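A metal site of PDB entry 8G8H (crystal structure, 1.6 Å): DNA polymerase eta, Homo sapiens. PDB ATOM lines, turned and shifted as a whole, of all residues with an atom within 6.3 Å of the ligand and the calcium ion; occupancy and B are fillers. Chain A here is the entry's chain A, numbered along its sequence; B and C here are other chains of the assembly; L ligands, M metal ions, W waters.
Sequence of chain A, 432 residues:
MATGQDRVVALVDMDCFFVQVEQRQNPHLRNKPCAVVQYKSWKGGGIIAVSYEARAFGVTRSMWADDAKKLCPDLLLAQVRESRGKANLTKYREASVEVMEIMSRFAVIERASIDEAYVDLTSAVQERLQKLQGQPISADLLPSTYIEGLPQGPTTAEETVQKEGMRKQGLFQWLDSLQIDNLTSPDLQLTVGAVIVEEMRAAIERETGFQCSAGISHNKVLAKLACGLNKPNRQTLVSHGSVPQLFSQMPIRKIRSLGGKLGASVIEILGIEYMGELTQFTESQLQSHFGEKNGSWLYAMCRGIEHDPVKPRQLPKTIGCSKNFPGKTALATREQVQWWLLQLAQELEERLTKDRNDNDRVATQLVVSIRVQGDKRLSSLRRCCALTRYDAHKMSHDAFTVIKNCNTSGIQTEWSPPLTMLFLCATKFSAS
The side-chain hydroxyl of Tyr 52 is in hydrogen-bond range of an oxygen (O4) of the ligand (2.8 Å).
N3 of DC 4 of chain B lies within hydrogen-bond range of N1 of the ligand (2.8 Å).
N of Cys 16 sits at hydrogen-bond distance from O4 of the ligand (2.8 Å).
O4 of DT 3 of chain B sits close to a nitrogen (N1) of the ligand (3.5 Å).
O4 of the ligand is in salt-bridge range of NH2 of Arg 55 (3.2 Å).
The guanidinium group of Arg 61 lies within salt-bridge range of an oxygen (O6) of the ligand (3.1 Å).
O7 of the ligand lies close to N of Phe 17, 3.1 Å away.
An oxygen (O4) of the ligand lies within salt-bridge range of the side-chain amino group of Lys 231.
The backbone NH of Asp 115 sits close to the side-chain hydroxyl of Ser 113 (3.2 Å).
NZ of Lys 231 lies within hydrogen-bond range of O of Asp 13.
OE2 of Glu 116 lies close to OD2 of Asp 13 (2.6 Å).
The side-chain amino group (NZ) of Lys 224 lies within salt-bridge range of the side-chain carboxylate (OD2) of Asp 13, 3.6 Å away.
NH1 of Arg 55 sits at hydrogen-bond distance from OH of Tyr 52 (3.2 Å).
The guanidinium group of Arg 55 sits at hydrogen-bond distance from the backbone carbonyl oxygen of Val 50, 2.9 Å away.
OG of Ser 113 is in hydrogen-bond range of O3' of DG 8 of chain C, at 2.6 Å.
OP1 of DG 8 of chain C lies within salt-bridge range of the side-chain amino group (NZ) of Lys 224, at 3.4 Å.
A nitrogen (N4) of the ligand sits close to N3 of DG 8 of chain C (3.3 Å).
Asp 15 touches the ligand (CA to O4, 3.6 Å).
Phe 18 touches the ligand (CZ to O5, 3.2 Å).
Ile 48 touches the ligand.
Ala 49 touches the ligand (CB to O3, 3.9 Å).
Ile 114 touches the ligand (CG2 to C8, 3.9 Å).
DC 5 of chain B touches the ligand.
Hydrophobic or aromatic side chains within 4 Å of the ligand: Phe 18, Ala 49, Tyr 52 and Ile 114.
Of the 25 residues printed, 18 come within 4 Å of the ligand.
The nearest printed residue that does not touch the ligand is Glu 116 (4.5 Å).
Of the 25 residues printed, 3 come within 4 Å of the calcium ion.
The side-chain carboxylate (OD2) of Asp 115 binds the calcium ion.
The calcium ion is bound by the side-chain carboxylate (OD1) of Asp 13 (2.2 Å).
An oxygen (O12) of the ligand is bound to the calcium ion, 2.2 Å away.
The calcium ion is bound by the backbone carbonyl oxygen (O) of Met 14 (2.3 Å).
An oxygen (O2) of the ligand binds the calcium ion (2.3 Å).
The calcium ion is bound by O7 of the ligand (2.3 Å).
The calcium ion has six donor atoms within binding distance.
Water W5 bridges O8 of the ligand and NH1 of Arg 61.
Water W3 lies within hydrogen-bond range of an oxygen (O9) of the ligand (2.5 Å), the backbone NH of Phe 18 (2.8 Å) and the backbone NH of Phe 17 (3.2 Å).
Water W4 lies within hydrogen-bond range of O3 of the ligand (2.5 Å), N of Val 50 (2.8 Å) and NH2 of Arg 55 (2.9 Å).
Water W1 lies within hydrogen-bond range of the backbone carbonyl oxygen of Ile 48 (2.7 Å), the guanidinium group of Arg 61 (2.9 Å) and an oxygen (O3) of the ligand (3.1 Å).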
ATOM      1  N   ASP A  13      -5.312  -4.739 -12.572  1.00  0.00           N
ATOM      2  CA  ASP A  13      -5.306  -6.141 -12.160  1.00  0.00           C
ATOM      3  C   ASP A  13      -5.844  -6.221 -10.728  1.00  0.00           C
ATOM      4  O   ASP A  13      -5.239  -5.666  -9.809  1.00  0.00           O
ATOM      5  CB  ASP A  13      -3.872  -6.702 -12.243  1.00  0.00           C
ATOM      6  CG  ASP A  13      -3.778  -8.177 -11.985  1.00  0.00           C
ATOM      7  OD1 ASP A  13      -4.339  -8.647 -11.008  1.00  0.00           O
ATOM      8  OD2 ASP A  13      -3.058  -8.865 -12.733  1.00  0.00           O
ATOM      9  N   MET A  14      -6.972  -6.911 -10.532  1.00  0.00           N
ATOM     10  CA  MET A  14      -7.533  -7.001  -9.191  1.00  0.00           C
ATOM     11  C   MET A  14      -6.586  -7.809  -8.295  1.00  0.00           C
ATOM     12  O   MET A  14      -6.082  -8.854  -8.717  1.00  0.00           O
ATOM     13  CB  MET A  14      -8.907  -7.662  -9.234  1.00  0.00           C
ATOM     14  CG  MET A  14      -9.919  -6.920 -10.085  1.00  0.00           C
ATOM     15  SD  MET A  14     -10.022  -5.151  -9.925  1.00  0.00           S
ATOM     16  CE  MET A  14     -10.794  -5.031  -8.314  1.00  0.00           C
ATOM     17  N   ASP A  15      -6.310  -7.321  -7.092  1.00  0.00           N
ATOM     18  CA  ASP A  15      -5.450  -8.058  -6.170  1.00  0.00           C
ATOM     19  C   ASP A  15      -6.209  -9.280  -5.653  1.00  0.00           C
ATOM     20  O   ASP A  15      -7.374  -9.173  -5.286  1.00  0.00           O
ATOM     21  CB  ASP A  15      -5.065  -7.175  -4.997  1.00  0.00           C
ATOM     22  CG  ASP A  15      -4.251  -5.960  -5.420  1.00  0.00           C
ATOM     23  OD1 ASP A  15      -3.506  -6.070  -6.395  1.00  0.00           O
ATOM     24  OD2 ASP A  15      -4.405  -4.900  -4.780  1.00  0.00           O
ATOM     25  N   CYS A  16      -5.515 -10.424  -5.564  1.00  0.00           N
ATOM     26  CA  CYS A  16      -6.104 -11.705  -5.122  1.00  0.00           C
ATOM     27  C   CYS A  16      -7.628 -11.748  -5.261  1.00  0.00           C
ATOM     28  O   CYS A  16      -8.345 -11.801  -4.252  1.00  0.00           O
ATOM     29  CB  CYS A  16      -5.702 -12.014  -3.665  1.00  0.00           C
ATOM     30  SG  CYS A  16      -5.911 -10.724  -2.406  1.00  0.00           S
ATOM     31  N   PHE A  17      -8.119 -11.719  -6.501  1.00  0.00           N
ATOM     32  CA  PHE A  17      -9.491 -11.287  -6.749  1.00  0.00           C
ATOM     33  C   PHE A  17     -10.506 -12.172  -6.045  1.00  0.00           C
ATOM     34  O   PHE A  17     -11.404 -11.661  -5.366  1.00  0.00           O
ATOM     35  CB  PHE A  17      -9.772 -11.239  -8.234  1.00  0.00           C
ATOM     36  CG  PHE A  17     -11.133 -10.666  -8.570  1.00  0.00           C
ATOM     37  CD1 PHE A  17     -11.603  -9.546  -7.919  1.00  0.00           C
ATOM     38  CD2 PHE A  17     -11.949 -11.310  -9.487  1.00  0.00           C
ATOM     39  CE1 PHE A  17     -12.883  -9.028  -8.200  1.00  0.00           C
ATOM     40  CE2 PHE A  17     -13.229 -10.804  -9.776  1.00  0.00           C
ATOM     41  CZ  PHE A  17     -13.683  -9.670  -9.134  1.00  0.00           C
ATOM     42  N   PHE A  18     -10.419 -13.499  -6.213  1.00  0.00           N
ATOM     43  CA  PHE A  18     -11.453 -14.363  -5.635  1.00  0.00           C
ATOM     44  C   PHE A  18     -11.501 -14.220  -4.111  1.00  0.00           C
ATOM     45  O   PHE A  18     -12.575 -14.297  -3.490  1.00  0.00           O
ATOM     46  CB  PHE A  18     -11.230 -15.824  -6.013  1.00  0.00           C
ATOM     47  CG  PHE A  18     -11.550 -16.165  -7.462  1.00  0.00           C
ATOM     48  CD1 PHE A  18     -11.729 -15.186  -8.422  1.00  0.00           C
ATOM     49  CD2 PHE A  18     -11.691 -17.494  -7.830  1.00  0.00           C
ATOM     50  CE1 PHE A  18     -12.015 -15.532  -9.753  1.00  0.00           C
ATOM     51  CE2 PHE A  18     -11.992 -17.843  -9.146  1.00  0.00           C
ATOM     52  CZ  PHE A  18     -12.160 -16.859 -10.099  1.00  0.00           C
ATOM     53  N   VAL A  19     -10.328 -14.059  -3.494  1.00  0.00           N
ATOM     54  CA  VAL A  19     -10.247 -13.827  -2.057  1.00  0.00           C
ATOM     55  C   VAL A  19     -10.959 -12.532  -1.676  1.00  0.00           C
ATOM     56  O   VAL A  19     -11.730 -12.498  -0.701  1.00  0.00           O
ATOM     57  CB  VAL A  19      -8.774 -13.810  -1.594  1.00  0.00           C
ATOM     58  CG1 VAL A  19      -8.638 -13.187  -0.210  1.00  0.00           C
ATOM     59  CG2 VAL A  19      -8.242 -15.232  -1.587  1.00  0.00           C
ATOM     60  N   ILE A  48      -7.089 -21.789  -5.435  1.00  0.00           N
ATOM     61  CA  ILE A  48      -7.124 -20.982  -6.650  1.00  0.00           C
ATOM     62  C   ILE A  48      -6.854 -19.508  -6.416  1.00  0.00           C
ATOM     63  O   ILE A  48      -6.578 -18.791  -7.385  1.00  0.00           O
ATOM     64  CB  ILE A  48      -8.436 -21.183  -7.440  1.00  0.00           C
ATOM     65  CG1 ILE A  48      -9.666 -20.751  -6.656  1.00  0.00           C
ATOM     66  CG2 ILE A  48      -8.583 -22.658  -7.871  1.00  0.00           C
ATOM     67  CD1 ILE A  48     -10.939 -21.267  -7.292  1.00  0.00           C
ATOM     68  N   ALA A  49      -6.885 -19.023  -5.185  1.00  0.00           N
ATOM     69  CA  ALA A  49      -6.524 -17.645  -4.899  1.00  0.00           C
ATOM     70  C   ALA A  49      -6.075 -17.557  -3.451  1.00  0.00           C
ATOM     71  O   ALA A  49      -6.570 -18.293  -2.604  1.00  0.00           O
ATOM     72  CB  ALA A  49      -7.691 -16.687  -5.172  1.00  0.00           C
ATOM     73  N   VAL A  50      -5.116 -16.667  -3.176  1.00  0.00           N
ATOM     74  CA  VAL A  50      -4.426 -16.611  -1.880  1.00  0.00           C
ATOM     75  C   VAL A  50      -4.293 -15.151  -1.427  1.00  0.00           C
ATOM     76  O   VAL A  50      -3.760 -14.322  -2.167  1.00  0.00           O
ATOM     77  CB  VAL A  50      -3.029 -17.254  -1.956  1.00  0.00           C
ATOM     78  CG1 VAL A  50      -2.427 -17.331  -0.579  1.00  0.00           C
ATOM     79  CG2 VAL A  50      -3.072 -18.616  -2.590  1.00  0.00           C
ATOM     80  N   TYR A  52      -2.770 -11.930   0.590  1.00  0.00           N
ATOM     81  CA  TYR A  52      -1.377 -11.563   0.790  1.00  0.00           C
ATOM     82  C   TYR A  52      -0.871 -11.976   2.169  1.00  0.00           C
ATOM     83  O   TYR A  52       0.308 -12.337   2.302  1.00  0.00           O
ATOM     84  CB  TYR A  52      -1.198 -10.055   0.493  1.00  0.00           C
ATOM     85  CG  TYR A  52      -1.121  -9.839  -1.011  1.00  0.00           C
ATOM     86  CD1 TYR A  52      -2.261  -9.802  -1.801  1.00  0.00           C
ATOM     87  CD2 TYR A  52       0.113  -9.735  -1.646  1.00  0.00           C
ATOM     88  CE1 TYR A  52      -2.178  -9.644  -3.188  1.00  0.00           C
ATOM     89  CE2 TYR A  52       0.210  -9.584  -3.020  1.00  0.00           C
ATOM     90  CZ  TYR A  52      -0.937  -9.532  -3.794  1.00  0.00           C
ATOM     91  OH  TYR A  52      -0.829  -9.377  -5.162  1.00  0.00           O
ATOM     92  N   ARG A  55       0.156 -15.499   1.640  1.00  0.00           N
ATOM     93  CA  ARG A  55       1.360 -15.587   0.815  1.00  0.00           C
ATOM     94  C   ARG A  55       2.627 -15.430   1.643  1.00  0.00           C
ATOM     95  O   ARG A  55       3.670 -15.995   1.283  1.00  0.00           O
ATOM     96  CB  ARG A  55       1.311 -14.532  -0.289  1.00  0.00           C
ATOM     97  CG  ARG A  55       0.173 -14.761  -1.267  1.00  0.00           C
ATOM     98  CD  ARG A  55       0.178 -13.702  -2.347  1.00  0.00           C
ATOM     99  NE  ARG A  55      -1.095 -13.660  -3.053  1.00  0.00           N
ATOM    100  CZ  ARG A  55      -1.267 -13.120  -4.244  1.00  0.00           C
ATOM    101  NH1 ARG A  55      -0.259 -12.551  -4.903  1.00  0.00           N
ATOM    102  NH2 ARG A  55      -2.467 -13.163  -4.811  1.00  0.00           N
ATOM    103  N   ARG A  61      -1.169 -20.360  -5.223  1.00  0.00           N
ATOM    104  CA  ARG A  61      -2.077 -21.023  -6.148  1.00  0.00           C
ATOM    105  C   ARG A  61      -1.536 -22.373  -6.551  1.00  0.00           C
ATOM    106  O   ARG A  61      -0.321 -22.584  -6.621  1.00  0.00           O
ATOM    107  CB  ARG A  61      -2.273 -20.162  -7.395  1.00  0.00           C
ATOM    108  CG  ARG A  61      -3.576 -20.378  -8.109  1.00  0.00           C
ATOM    109  CD  ARG A  61      -3.671 -19.448  -9.299  1.00  0.00           C
ATOM    110  NE  ARG A  61      -2.366 -19.303  -9.939  1.00  0.00           N
ATOM    111  CZ  ARG A  61      -1.801 -18.144 -10.220  1.00  0.00           C
ATOM    112  NH1 ARG A  61      -2.373 -16.994  -9.901  1.00  0.00           N
ATOM    113  NH2 ARG A  61      -0.619 -18.137 -10.840  1.00  0.00           N
ATOM    114  N   LEU A  89     -18.153 -20.516 -11.227  1.00  0.00           N
ATOM    115  CA  LEU A  89     -17.434 -19.266 -11.021  1.00  0.00           C
ATOM    116  C   LEU A  89     -18.347 -18.046 -11.115  1.00  0.00           C
ATOM    117  O   LEU A  89     -17.831 -16.915 -11.124  1.00  0.00           O
ATOM    118  CB  LEU A  89     -16.305 -19.165 -12.066  1.00  0.00           C
ATOM    119  CG  LEU A  89     -15.179 -20.193 -11.884  1.00  0.00           C
ATOM    120  CD1 LEU A  89     -14.023 -19.936 -12.868  1.00  0.00           C
ATOM    121  CD2 LEU A  89     -14.692 -20.252 -10.453  1.00  0.00           C
ATOM    122  N   SER A 113      -9.036 -10.855 -18.847  1.00  0.00           N
ATOM    123  CA  SER A 113      -9.295 -12.051 -18.047  1.00  0.00           C
ATOM    124  C   SER A 113     -10.437 -11.700 -17.104  1.00  0.00           C
ATOM    125  O   SER A 113     -11.002 -10.604 -17.171  1.00  0.00           O
ATOM    126  CB  SER A 113      -8.044 -12.502 -17.285  1.00  0.00           C
ATOM    127  OG  SER A 113      -7.829 -11.652 -16.154  1.00  0.00           O
ATOM    128  N   ILE A 114     -10.765 -12.618 -16.194  1.00  0.00           N
ATOM    129  CA  ILE A 114     -11.840 -12.350 -15.246  1.00  0.00           C
ATOM    130  C   ILE A 114     -11.486 -11.166 -14.371  1.00  0.00           C
ATOM    131  O   ILE A 114     -12.371 -10.481 -13.842  1.00  0.00           O
ATOM    132  CB  ILE A 114     -12.130 -13.609 -14.418  1.00  0.00           C
ATOM    133  CG1 ILE A 114     -13.355 -13.406 -13.552  1.00  0.00           C
ATOM    134  CG2 ILE A 114     -10.927 -13.975 -13.556  1.00  0.00           C
ATOM    135  CD1 ILE A 114     -14.140 -14.684 -13.276  1.00  0.00           C
ATOM    136  N   ASP A 115     -10.188 -10.862 -14.200  1.00  0.00           N
ATOM    137  CA  ASP A 115      -9.857  -9.825 -13.243  1.00  0.00           C
ATOM    138  C   ASP A 115      -8.823  -8.812 -13.752  1.00  0.00           C
ATOM    139  O   ASP A 115      -8.272  -8.069 -12.933  1.00  0.00           O
ATOM    140  CB  ASP A 115      -9.396 -10.465 -11.947  1.00  0.00           C
ATOM    141  CG  ASP A 115      -7.940 -10.797 -11.938  1.00  0.00           C
ATOM    142  OD1 ASP A 115      -7.436 -11.255 -12.997  1.00  0.00           O
ATOM    143  OD2 ASP A 115      -7.307 -10.621 -10.873  1.00  0.00           O
ATOM    144  N   GLU A 116      -8.572  -8.735 -15.051  1.00  0.00           N
ATOM    145  CA  GLU A 116      -7.762  -7.644 -15.557  1.00  0.00           C
ATOM    146  C   GLU A 116      -8.352  -7.081 -16.837  1.00  0.00           C
ATOM    147  O   GLU A 116      -9.097  -7.740 -17.556  1.00  0.00           O
ATOM    148  CB  GLU A 116      -6.274  -7.995 -15.750  1.00  0.00           C
ATOM    149  CG  GLU A 116      -5.878  -9.367 -16.041  1.00  0.00           C
ATOM    150  CD  GLU A 116      -4.366  -9.501 -16.008  1.00  0.00           C
ATOM    151  OE1 GLU A 116      -3.752  -9.175 -17.031  1.00  0.00           O
ATOM    152  OE2 GLU A 116      -3.776  -9.884 -14.969  1.00  0.00           O
ATOM    153  N   LYS A 224       1.515  -4.162 -18.362  1.00  0.00           N
ATOM    154  CA  LYS A 224       1.391  -5.399 -17.605  1.00  0.00           C
ATOM    155  C   LYS A 224       2.596  -5.607 -16.701  1.00  0.00           C
ATOM    156  O   LYS A 224       2.449  -5.971 -15.522  1.00  0.00           O
ATOM    157  CB  LYS A 224       1.214  -6.566 -18.581  1.00  0.00           C
ATOM    158  CG  LYS A 224       1.247  -7.935 -17.944  1.00  0.00           C
ATOM    159  CD  LYS A 224       0.123  -8.119 -16.953  1.00  0.00           C
ATOM    160  CE  LYS A 224       0.018  -9.598 -16.577  1.00  0.00           C
ATOM    161  NZ  LYS A 224      -0.826  -9.819 -15.372  1.00  0.00           N
ATOM    162  N   LYS A 231       2.808  -4.458  -6.170  1.00  0.00           N
ATOM    163  CA  LYS A 231       1.557  -5.079  -5.753  1.00  0.00           C
ATOM    164  C   LYS A 231       1.586  -5.309  -4.245  1.00  0.00           C
ATOM    165  O   LYS A 231       2.654  -5.468  -3.652  1.00  0.00           O
ATOM    166  CB  LYS A 231       1.356  -6.413  -6.486  1.00  0.00           C
ATOM    167  CG  LYS A 231       0.443  -6.369  -7.736  1.00  0.00           C
ATOM    168  CD  LYS A 231      -0.092  -7.768  -8.163  1.00  0.00           C
ATOM    169  CE  LYS A 231      -1.295  -7.676  -9.123  1.00  0.00           C
ATOM    170  NZ  LYS A 231      -2.675  -7.551  -8.465  1.00  0.00           N
ATOM    171  N   PRO A 232       0.452  -5.307  -3.529  1.00  0.00           N
ATOM    172  CA  PRO A 232      -0.926  -4.976  -3.908  1.00  0.00           C
ATOM    173  C   PRO A 232      -1.283  -3.523  -3.674  1.00  0.00           C
ATOM    174  O   PRO A 232      -0.549  -2.802  -2.987  1.00  0.00           O
ATOM    175  CB  PRO A 232      -1.744  -5.864  -2.960  1.00  0.00           C
ATOM    176  CG  PRO A 232      -0.959  -5.792  -1.693  1.00  0.00           C
ATOM    177  CD  PRO A 232       0.512  -5.714  -2.109  1.00  0.00           C
ATOM    178  P    DT B   3      -0.456 -32.724  -9.381  1.00  0.00           P
ATOM    179  OP1  DT B   3      -0.040 -33.239 -10.713  1.00  0.00           O
ATOM    180  OP2  DT B   3       0.406 -32.878  -8.188  1.00  0.00           O
ATOM    181  O5'  DT B   3      -0.778 -31.169  -9.537  1.00  0.00           O
ATOM    182  C5'  DT B   3      -1.443 -30.689 -10.707  1.00  0.00           C
ATOM    183  C4'  DT B   3      -2.883 -30.352 -10.384  1.00  0.00           C
ATOM    184  O4'  DT B   3      -2.986 -28.957  -9.984  1.00  0.00           O
ATOM    185  C3'  DT B   3      -3.873 -30.527 -11.537  1.00  0.00           C
ATOM    186  O3'  DT B   3      -5.136 -30.844 -10.979  1.00  0.00           O
ATOM    187  C2'  DT B   3      -3.893 -29.118 -12.103  1.00  0.00           C
ATOM    188  C1'  DT B   3      -3.973 -28.354 -10.800  1.00  0.00           C
ATOM    189  N1   DT B   3      -3.734 -26.867 -10.903  1.00  0.00           N
ATOM    190  C2   DT B   3      -4.638 -26.011 -10.302  1.00  0.00           C
ATOM    191  O2   DT B   3      -5.617 -26.414  -9.689  1.00  0.00           O
ATOM    192  N3   DT B   3      -4.366 -24.678 -10.436  1.00  0.00           N
ATOM    193  C4   DT B   3      -3.295 -24.109 -11.115  1.00  0.00           C
ATOM    194  O4   DT B   3      -3.133 -22.887 -11.180  1.00  0.00           O
ATOM    195  C5   DT B   3      -2.370 -25.056 -11.729  1.00  0.00           C
ATOM    196  C7   DT B   3      -1.168 -24.560 -12.480  1.00  0.00           C
ATOM    197  C6   DT B   3      -2.632 -26.372 -11.595  1.00  0.00           C
ATOM    198  P    DC B   4      -6.207 -31.758 -11.764  1.00  0.00           P
ATOM    199  OP1  DC B   4      -6.601 -32.798 -10.775  1.00  0.00           O
ATOM    200  OP2  DC B   4      -5.668 -32.157 -13.080  1.00  0.00           O
ATOM    201  O5'  DC B   4      -7.432 -30.756 -11.980  1.00  0.00           O
ATOM    202  C5'  DC B   4      -7.872 -29.922 -10.897  1.00  0.00           C
ATOM    203  C4'  DC B   4      -8.677 -28.732 -11.393  1.00  0.00           C
ATOM    204  O4'  DC B   4      -7.788 -27.626 -11.706  1.00  0.00           O
ATOM    205  C3'  DC B   4      -9.492 -28.993 -12.658  1.00  0.00           C
ATOM    206  O3'  DC B   4     -10.739 -28.364 -12.546  1.00  0.00           O
ATOM    207  C2'  DC B   4      -8.635 -28.344 -13.754  1.00  0.00           C
ATOM    208  C1'  DC B   4      -8.072 -27.152 -13.004  1.00  0.00           C
ATOM    209  N1   DC B   4      -6.813 -26.594 -13.609  1.00  0.00           N
ATOM    210  C2   DC B   4      -6.618 -25.218 -13.634  1.00  0.00           C
ATOM    211  O2   DC B   4      -7.496 -24.492 -13.169  1.00  0.00           O
ATOM    212  N3   DC B   4      -5.480 -24.718 -14.173  1.00  0.00           N
ATOM    213  C4   DC B   4      -4.553 -25.540 -14.668  1.00  0.00           C
ATOM    214  N4   DC B   4      -3.448 -25.000 -15.195  1.00  0.00           N
ATOM    215  C5   DC B   4      -4.732 -26.959 -14.653  1.00  0.00           C
ATOM    216  C6   DC B   4      -5.867 -27.438 -14.121  1.00  0.00           C
ATOM    217  P    DC B   5     -11.903 -28.716 -13.584  1.00  0.00           P
ATOM    218  OP1  DC B   5     -13.178 -28.137 -13.123  1.00  0.00           O
ATOM    219  OP2  DC B   5     -11.794 -30.137 -13.957  1.00  0.00           O
ATOM    220  O5'  DC B   5     -11.458 -27.958 -14.901  1.00  0.00           O
ATOM    221  C5'  DC B   5     -12.405 -27.273 -15.632  1.00  0.00           C
ATOM    222  C4'  DC B   5     -12.258 -25.778 -15.442  1.00  0.00           C
ATOM    223  O4'  DC B   5     -10.868 -25.444 -15.244  1.00  0.00           O
ATOM    224  C3'  DC B   5     -12.711 -24.993 -16.648  1.00  0.00           C
ATOM    225  O3'  DC B   5     -13.894 -24.352 -16.393  1.00  0.00           O
ATOM    226  C2'  DC B   5     -11.591 -23.979 -16.916  1.00  0.00           C
ATOM    227  C1'  DC B   5     -10.659 -24.137 -15.735  1.00  0.00           C
ATOM    228  N1   DC B   5      -9.286 -24.028 -16.170  1.00  0.00           N
ATOM    229  C2   DC B   5      -8.699 -22.755 -16.314  1.00  0.00           C
ATOM    230  O2   DC B   5      -9.362 -21.749 -16.027  1.00  0.00           O
ATOM    231  N3   DC B   5      -7.433 -22.678 -16.746  1.00  0.00           N
ATOM    232  C4   DC B   5      -6.754 -23.784 -17.046  1.00  0.00           C
ATOM    233  N4   DC B   5      -5.501 -23.644 -17.475  1.00  0.00           N
ATOM    234  C5   DC B   5      -7.329 -25.076 -16.925  1.00  0.00           C
ATOM    235  C6   DC B   5      -8.590 -25.144 -16.492  1.00  0.00           C
ATOM    236  P    DG C   8      -0.409 -13.849 -16.803  1.00  0.00           P
ATOM    237  OP1  DG C   8       0.464 -12.683 -16.559  1.00  0.00           O
ATOM    238  OP2  DG C   8      -0.063 -15.163 -16.185  1.00  0.00           O
ATOM    239  O5'  DG C   8      -1.913 -13.521 -16.354  1.00  0.00           O
ATOM    240  C5'  DG C   8      -2.804 -12.824 -17.217  1.00  0.00           C
ATOM    241  C4'  DG C   8      -4.230 -13.040 -16.740  1.00  0.00           C
ATOM    242  O4'  DG C   8      -4.673 -14.352 -17.136  1.00  0.00           O
ATOM    243  C3'  DG C   8      -4.396 -12.979 -15.216  1.00  0.00           C
ATOM    244  O3'  DG C   8      -5.626 -12.335 -14.878  1.00  0.00           O
ATOM    245  C2'  DG C   8      -4.388 -14.451 -14.800  1.00  0.00           C
ATOM    246  C1'  DG C   8      -4.997 -15.144 -16.016  1.00  0.00           C
ATOM    247  N9   DG C   8      -4.494 -16.495 -16.252  1.00  0.00           N
ATOM    248  C8   DG C   8      -3.193 -16.880 -16.359  1.00  0.00           C
ATOM    249  N7   DG C   8      -3.026 -18.149 -16.596  1.00  0.00           N
ATOM    250  C5   DG C   8      -4.314 -18.640 -16.633  1.00  0.00           C
ATOM    251  C6   DG C   8      -4.775 -19.963 -16.844  1.00  0.00           C
ATOM    252  O6   DG C   8      -4.097 -20.976 -17.040  1.00  0.00           O
ATOM    253  N1   DG C   8      -6.163 -20.034 -16.798  1.00  0.00           N
ATOM    254  C2   DG C   8      -6.991 -18.961 -16.579  1.00  0.00           C
ATOM    255  N2   DG C   8      -8.310 -19.206 -16.581  1.00  0.00           N
ATOM    256  N3   DG C   8      -6.580 -17.724 -16.381  1.00  0.00           N
ATOM    257  C4   DG C   8      -5.229 -17.633 -16.423  1.00  0.00           C
HETATM  258  C1  LIG L   1      -6.649 -21.608 -13.683  1.00  0.00           C
HETATM  259  C2  LIG L   1      -5.976 -19.384 -13.320  1.00  0.00           C
HETATM  260  C3  LIG L   1      -4.693 -19.758 -13.354  1.00  0.00           C
HETATM  261  C4  LIG L   1      -4.370 -21.044 -13.564  1.00  0.00           C
HETATM  262  O1  LIG L   1      -3.056 -21.389 -13.599  1.00  0.00           O
HETATM  263  C5  LIG L   1      -7.362 -17.365 -13.026  1.00  0.00           C
HETATM  264  C6  LIG L   1      -8.134 -17.625 -11.715  1.00  0.00           C
HETATM  265  C7  LIG L   1      -7.571 -16.511 -10.868  1.00  0.00           C
HETATM  266  C8  LIG L   1      -7.711 -15.383 -11.847  1.00  0.00           C
HETATM  267  C9  LIG L   1      -6.870 -14.185 -11.392  1.00  0.00           C
HETATM  268  C10 LIG L   1      -4.784 -17.617 -13.024  1.00  0.00           C
HETATM  269  N1  LIG L   1      -5.320 -21.973 -13.714  1.00  0.00           N
HETATM  270  N2  LIG L   1      -6.972 -20.276 -13.479  1.00  0.00           N
HETATM  271  N3  LIG L   1      -3.959 -18.653 -13.170  1.00  0.00           N
HETATM  272  N4  LIG L   1      -6.034 -18.072 -13.113  1.00  0.00           N
HETATM  273  O2  LIG L   1      -4.498 -12.327 -11.285  1.00  0.00           O
HETATM  274  O3  LIG L   1      -5.521 -14.305  -7.307  1.00  0.00           O
HETATM  275  O4  LIG L   1      -2.890 -10.518  -6.626  1.00  0.00           O
HETATM  276  O5  LIG L   1      -9.555 -17.371 -11.887  1.00  0.00           O
HETATM  277  O6  LIG L   1      -3.049 -14.448 -11.533  1.00  0.00           O
HETATM  278  O7  LIG L   1      -5.860 -12.089  -8.592  1.00  0.00           O
HETATM  279  O8  LIG L   1      -1.462 -12.170  -7.904  1.00  0.00           O
HETATM  280  O9  LIG L   1      -8.449 -16.280  -9.727  1.00  0.00           O
HETATM  281  O10 LIG L   1      -4.232 -14.029  -9.354  1.00  0.00           O
HETATM  282  O11 LIG L   1      -3.626 -12.631  -7.377  1.00  0.00           O
HETATM  283  O12 LIG L   1      -3.345 -10.942  -9.068  1.00  0.00           O
HETATM  284  O13 LIG L   1      -7.067 -15.918 -13.008  1.00  0.00           O
HETATM  285  O14 LIG L   1      -5.506 -14.638 -11.401  1.00  0.00           O
HETATM  286  P1  LIG L   1      -4.240 -13.755 -10.955  1.00  0.00           P
HETATM  287  P2  LIG L   1      -4.940 -13.195  -8.139  1.00  0.00           P
HETATM  288  P3  LIG L   1      -2.693 -11.345  -7.808  1.00  0.00           P
HETATM  289 CA    CA M   1      -5.249 -10.466 -10.139  1.00  0.00          CA
HETATM  290  O   HOH W   1      -4.975 -17.003  -8.703  1.00  0.00           O
HETATM  291  O   HOH W   2      -1.553 -10.970 -11.642  1.00  0.00           O
HETATM  292  O   HOH W   3      -8.385 -14.665  -7.783  1.00  0.00           O
HETATM  293  O   HOH W   4      -4.131 -15.451  -5.519  1.00  0.00           O
HETATM  294  O   HOH W   5      -0.864 -14.410  -8.569  1.00  0.00           O
